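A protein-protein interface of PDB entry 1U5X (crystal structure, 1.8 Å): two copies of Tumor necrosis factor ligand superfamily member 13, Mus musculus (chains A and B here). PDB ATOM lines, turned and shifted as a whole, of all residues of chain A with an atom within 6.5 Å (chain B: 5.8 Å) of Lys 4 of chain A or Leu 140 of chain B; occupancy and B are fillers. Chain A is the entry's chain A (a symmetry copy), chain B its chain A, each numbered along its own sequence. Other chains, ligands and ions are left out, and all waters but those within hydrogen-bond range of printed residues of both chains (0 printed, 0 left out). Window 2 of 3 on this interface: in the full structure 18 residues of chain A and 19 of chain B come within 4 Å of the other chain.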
ATOM      1  N   LYS A   4     -25.761 -11.355  -9.039  1.00  0.00           N
ATOM      2  CA  LYS A   4     -24.598 -12.284  -8.870  1.00  0.00           C
ATOM      3  C   LYS A   4     -25.066 -13.688  -8.456  1.00  0.00           C
ATOM      4  O   LYS A   4     -25.543 -13.883  -7.342  1.00  0.00           O
ATOM      5  CB  LYS A   4     -23.641 -11.721  -7.841  1.00  0.00           C
ATOM      6  N   HIS A   5     -24.901 -14.660  -9.353  1.00  0.00           N
ATOM      7  CA  HIS A   5     -25.495 -15.981  -9.203  1.00  0.00           C
ATOM      8  C   HIS A   5     -24.612 -16.954  -8.412  1.00  0.00           C
ATOM      9  O   HIS A   5     -23.402 -16.919  -8.526  1.00  0.00           O
ATOM     10  CB  HIS A   5     -25.738 -16.610 -10.585  1.00  0.00           C
ATOM     11  CG  HIS A   5     -26.766 -15.899 -11.402  1.00  0.00           C
ATOM     12  ND1 HIS A   5     -27.808 -16.561 -12.017  1.00  0.00           N
ATOM     13  CD2 HIS A   5     -26.919 -14.589 -11.709  1.00  0.00           C
ATOM     14  CE1 HIS A   5     -28.554 -15.691 -12.669  1.00  0.00           C
ATOM     15  NE2 HIS A   5     -28.044 -14.486 -12.491  1.00  0.00           N
ATOM     16  N   SER A   6     -25.234 -17.858  -7.662  1.00  0.00           N
ATOM     17  CA  SER A   6     -24.520 -18.981  -7.060  1.00  0.00           C
ATOM     18  C   SER A   6     -24.221 -20.050  -8.114  1.00  0.00           C
ATOM     19  O   SER A   6     -25.062 -20.358  -8.959  1.00  0.00           O
ATOM     20  CB  SER A   6     -25.364 -19.593  -5.960  1.00  0.00           C
ATOM     21  OG  SER A   6     -25.644 -18.611  -4.995  1.00  0.00           O
ATOM     22  N   VAL A   7     -23.023 -20.620  -8.058  1.00  0.00           N
ATOM     23  CA  VAL A   7     -22.591 -21.577  -9.066  1.00  0.00           C
ATOM     24  C   VAL A   7     -21.722 -22.681  -8.483  1.00  0.00           C
ATOM     25  O   VAL A   7     -21.117 -22.519  -7.406  1.00  0.00           O
ATOM     26  CB  VAL A   7     -21.847 -20.908 -10.274  1.00  0.00           C
ATOM     27  CG1 VAL A   7     -22.605 -19.645 -10.791  1.00  0.00           C
ATOM     28  CG2 VAL A   7     -20.459 -20.560  -9.934  1.00  0.00           C
ATOM     29  N   ARG A  34     -19.308 -20.551  -6.029  1.00  0.00           N
ATOM     30  CA  ARG A  34     -19.809 -19.328  -5.468  1.00  0.00           C
ATOM     31  C   ARG A  34     -21.138 -19.601  -4.776  1.00  0.00           C
ATOM     32  O   ARG A  34     -21.989 -20.316  -5.304  1.00  0.00           O
ATOM     33  CB  ARG A  34     -20.018 -18.261  -6.545  1.00  0.00           C
ATOM     34  CG  ARG A  34     -20.552 -16.971  -5.948  1.00  0.00           C
ATOM     35  CD  ARG A  34     -20.382 -15.752  -6.819  1.00  0.00           C
ATOM     36  NE  ARG A  34     -21.187 -15.847  -8.031  1.00  0.00           N
ATOM     37  CZ  ARG A  34     -21.017 -15.091  -9.112  1.00  0.00           C
ATOM     38  NH1 ARG A  34     -20.062 -14.169  -9.156  1.00  0.00           N
ATOM     39  NH2 ARG A  34     -21.800 -15.261 -10.162  1.00  0.00           N
ATOM     40  N   VAL A 138     -26.070 -23.534 -11.955  1.00  0.00           N
ATOM     41  CA  VAL A 138     -26.187 -22.105 -11.766  1.00  0.00           C
ATOM     42  C   VAL A 138     -27.583 -21.801 -11.233  1.00  0.00           C
ATOM     43  O   VAL A 138     -28.596 -22.071 -11.905  1.00  0.00           O
ATOM     44  CB  VAL A 138     -26.067 -21.327 -13.093  1.00  0.00           C
ATOM     45  CG1 VAL A 138     -26.205 -19.801 -12.847  1.00  0.00           C
ATOM     46  CG2 VAL A 138     -24.751 -21.682 -13.802  1.00  0.00           C
ATOM     47  N   LYS A 139     -27.640 -21.225 -10.046  1.00  0.00           N
ATOM     48  CA  LYS A 139     -28.901 -20.785  -9.508  1.00  0.00           C
ATOM     49  C   LYS A 139     -29.389 -19.574 -10.274  1.00  0.00           C
ATOM     50  O   LYS A 139     -28.640 -18.588 -10.485  1.00  0.00           O
ATOM     51  CB  LYS A 139     -28.792 -20.490  -8.019  1.00  0.00           C
ATOM     52  CG  LYS A 139     -30.147 -20.300  -7.357  1.00  0.00           C
ATOM     53  CD  LYS A 139     -29.978 -20.166  -5.861  1.00  0.00           C
ATOM     54  CE  LYS A 139     -31.051 -19.288  -5.231  1.00  0.00           C
ATOM     55  NZ  LYS A 139     -32.237 -20.044  -4.828  1.00  0.00           N
ATOM     56  N   LEU A 140     -30.649 -19.666 -10.719  1.00  0.00           N
ATOM     57  CA  LEU A 140     -31.274 -18.652 -11.564  1.00  0.00           C
ATOM     58  C   LEU A 140     -32.263 -17.782 -10.807  1.00  0.00           C
ATOM     59  O   LEU A 140     -32.643 -18.089  -9.674  1.00  0.00           O
ATOM     60  CB  LEU A 140     -31.959 -19.336 -12.759  1.00  0.00           C
ATOM     61  CG  LEU A 140     -31.036 -20.109 -13.689  1.00  0.00           C
ATOM     62  CD1 LEU A 140     -31.823 -20.778 -14.840  1.00  0.00           C
ATOM     63  CD2 LEU A 140     -29.895 -19.261 -14.238  1.00  0.00           C
ATOM     64  OXT LEU A 140     -32.694 -16.740 -11.324  1.00  0.00           O
ATOM     65  N   HIS B   5     -27.678  -9.171 -17.504  1.00  0.00           N
ATOM     66  CA  HIS B   5     -26.363  -9.766 -17.695  1.00  0.00           C
ATOM     67  C   HIS B   5     -25.636  -9.238 -18.938  1.00  0.00           C
ATOM     68  O   HIS B   5     -26.258  -8.973 -19.950  1.00  0.00           O
ATOM     69  CB  HIS B   5     -26.491 -11.290 -17.858  1.00  0.00           C
ATOM     70  CG  HIS B   5     -26.973 -11.991 -16.631  1.00  0.00           C
ATOM     71  ND1 HIS B   5     -26.334 -13.098 -16.114  1.00  0.00           N
ATOM     72  CD2 HIS B   5     -28.028 -11.752 -15.818  1.00  0.00           C
ATOM     73  CE1 HIS B   5     -26.974 -13.511 -15.038  1.00  0.00           C
ATOM     74  NE2 HIS B   5     -28.000 -12.706 -14.829  1.00  0.00           N
ATOM     75  N   ILE B  52     -17.236 -14.572 -13.465  1.00  0.00           N
ATOM     76  CA  ILE B  52     -17.673 -15.921 -13.772  1.00  0.00           C
ATOM     77  C   ILE B  52     -18.598 -15.883 -14.990  1.00  0.00           C
ATOM     78  O   ILE B  52     -19.533 -15.076 -15.058  1.00  0.00           O
ATOM     79  CB  ILE B  52     -18.374 -16.536 -12.520  1.00  0.00           C
ATOM     80  CG1 ILE B  52     -17.340 -16.742 -11.393  1.00  0.00           C
ATOM     81  CG2 ILE B  52     -19.067 -17.800 -12.869  1.00  0.00           C
ATOM     82  CD1 ILE B  52     -17.937 -17.218 -10.073  1.00  0.00           C
ATOM     83  N   TYR B  53     -18.314 -16.717 -15.986  1.00  0.00           N
ATOM     84  CA  TYR B  53     -19.033 -16.696 -17.242  1.00  0.00           C
ATOM     85  C   TYR B  53     -19.457 -18.063 -17.634  1.00  0.00           C
ATOM     86  O   TYR B  53     -18.706 -19.012 -17.490  1.00  0.00           O
ATOM     87  CB  TYR B  53     -18.095 -16.222 -18.358  1.00  0.00           C
ATOM     88  CG  TYR B  53     -17.654 -14.794 -18.242  1.00  0.00           C
ATOM     89  CD1 TYR B  53     -16.556 -14.436 -17.458  1.00  0.00           C
ATOM     90  CD2 TYR B  53     -18.296 -13.793 -18.973  1.00  0.00           C
ATOM     91  CE1 TYR B  53     -16.121 -13.113 -17.381  1.00  0.00           C
ATOM     92  CE2 TYR B  53     -17.862 -12.453 -18.898  1.00  0.00           C
ATOM     93  CZ  TYR B  53     -16.793 -12.125 -18.100  1.00  0.00           C
ATOM     94  OH  TYR B  53     -16.379 -10.824 -18.059  1.00  0.00           O
ATOM     95  N   LEU B  54     -20.670 -18.155 -18.155  1.00  0.00           N
ATOM     96  CA  LEU B  54     -21.072 -19.272 -18.981  1.00  0.00           C
ATOM     97  C   LEU B  54     -20.477 -19.065 -20.361  1.00  0.00           C
ATOM     98  O   LEU B  54     -20.659 -17.992 -20.970  1.00  0.00           O
ATOM     99  CB  LEU B  54     -22.590 -19.287 -19.077  1.00  0.00           C
ATOM    100  CG  LEU B  54     -23.191 -20.364 -19.985  1.00  0.00           C
ATOM    101  CD1 LEU B  54     -22.882 -21.765 -19.462  1.00  0.00           C
ATOM    102  CD2 LEU B  54     -24.727 -20.139 -20.116  1.00  0.00           C
ATOM    103  N   VAL B 106     -19.182 -23.281 -16.959  1.00  0.00           N
ATOM    104  CA  VAL B 106     -19.040 -22.047 -16.215  1.00  0.00           C
ATOM    105  C   VAL B 106     -17.637 -21.934 -15.668  1.00  0.00           C
ATOM    106  O   VAL B 106     -17.168 -22.852 -15.013  1.00  0.00           O
ATOM    107  CB  VAL B 106     -20.036 -21.947 -15.073  1.00  0.00           C
ATOM    108  CG1 VAL B 106     -19.843 -20.675 -14.323  1.00  0.00           C
ATOM    109  CG2 VAL B 106     -21.424 -21.962 -15.630  1.00  0.00           C
ATOM    110  N   VAL B 138     -21.927 -15.463 -21.275  1.00  0.00           N
ATOM    111  CA  VAL B 138     -22.834 -14.736 -20.415  1.00  0.00           C
ATOM    112  C   VAL B 138     -22.167 -14.551 -19.056  1.00  0.00           C
ATOM    113  O   VAL B 138     -21.858 -15.535 -18.358  1.00  0.00           O
ATOM    114  CB  VAL B 138     -24.134 -15.519 -20.140  1.00  0.00           C
ATOM    115  CG1 VAL B 138     -25.075 -14.708 -19.210  1.00  0.00           C
ATOM    116  CG2 VAL B 138     -24.818 -15.899 -21.463  1.00  0.00           C
ATOM    117  N   LYS B 139     -21.965 -13.304 -18.673  1.00  0.00           N
ATOM    118  CA  LYS B 139     -21.457 -13.019 -17.356  1.00  0.00           C
ATOM    119  C   LYS B 139     -22.521 -13.312 -16.322  1.00  0.00           C
ATOM    120  O   LYS B 139     -23.690 -12.866 -16.440  1.00  0.00           O
ATOM    121  CB  LYS B 139     -20.967 -11.581 -17.253  1.00  0.00           C
ATOM    122  CG  LYS B 139     -20.170 -11.322 -15.986  1.00  0.00           C
ATOM    123  CD  LYS B 139     -19.585  -9.928 -16.020  1.00  0.00           C
ATOM    124  CE  LYS B 139     -19.436  -9.327 -14.628  1.00  0.00           C
ATOM    125  NZ  LYS B 139     -18.146  -9.637 -14.012  1.00  0.00           N
ATOM    126  N   LEU B 140     -22.119 -14.097 -15.313  1.00  0.00           N
ATOM    127  CA  LEU B 140     -23.018 -14.580 -14.269  1.00  0.00           C
ATOM    128  C   LEU B 140     -22.837 -13.849 -12.950  1.00  0.00           C
ATOM    129  O   LEU B 140     -21.866 -13.110 -12.761  1.00  0.00           O
ATOM    130  CB  LEU B 140     -22.814 -16.092 -14.081  1.00  0.00           C
ATOM    131  CG  LEU B 140     -23.126 -16.952 -15.297  1.00  0.00           C
ATOM    132  CD1 LEU B 140     -22.866 -18.450 -15.014  1.00  0.00           C
ATOM    133  CD2 LEU B 140     -24.538 -16.742 -15.831  1.00  0.00           C
ATOM    134  OXT LEU B 140     -23.677 -13.982 -12.047  1.00  0.00           O
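His 5 of chain A touches its own counterpart, His 5 of chain B.
His 5 of chain A touches Leu 140 of chain B, but with the chains exchanged Leu 140 of chain A does not touch His 5 of chain B (6.5 Å).
Val 138 of chain A touches Leu 140 of chain B, but with the chains exchanged Leu 140 of chain A does not touch Val 138 of chain B (8.3 Å).
Positions printed for both chains: 5, 138, 139 and 140.
Of the 7 pairs that touch across the chains among the printed residues, 1 has its exchanged pair printed and touching as well.
A ring nitrogen (NE2) of His 5 of chain A sits close to a ring nitrogen (NE2) of His 5 of chain B (2.9 Å).
The chain-end carboxylate of Leu 140 of chain B lies within hydrogen-bond range of the backbone NH of His 5 of chain A.
OXT of Leu 140 of chain B is in salt-bridge range of NH2 of Arg 34 of chain A, 3.0 Å away.
O of Lys 139 of chain B sits at hydrogen-bond distance from ND1 of His 5 of chain B, at 2.7 Å.
The backbone carbonyl oxygen (O) of Ile 52 of chain B sits at hydrogen-bond distance from the backbone NH (N) of Leu 140 of chain B (2.8 Å).
O of His 5 of chain A lies within hydrogen-bond range of NE of Arg 34 of chain A (2.5 Å).
A ring nitrogen (ND1) of His 5 of chain A lies within hydrogen-bond range of the backbone carbonyl oxygen (O) of Lys 139 of chain A (2.7 Å).
The backbone carbonyl oxygen (O) of Arg 34 of chain A lies within hydrogen-bond range of the backbone NH (N) of Val 7 of chain A, at 3.0 Å.
Hydrophobic or aromatic side chains of chain A within 4 Å of the printed part of chain B: His 5 and Val 138.
Printed residues of chain B that touch a printed residue of chain A: His 5, Ile 52, Val 106 and Leu 140.
Hydrophobic or aromatic side chains of chain B within 4 Å of the printed part of chain A: His 5, Ile 52, Val 106 and Leu 140.
Val 7 of chain A touches none of the printed residues of chain B.
Of the printed residues of chain A, Ile 52 of chain B touches Arg 34.
Printed residues of chain A within 4 Å of Val 106 of chain B: Val 138 (3.8 Å).
Leu 140 of chain B touches four residues of chain A.
Lys 4 of chain A touches Leu 140 of chain B (CA to OXT, 3.7 Å).
Ile 52 of chain B touches Arg 34 of chain A (CD1 to NH1, 3.8 Å).
Val 138 of chain A touches Val 106 of chain B.
Val 138 of chain A touches Leu 140 of chain B.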
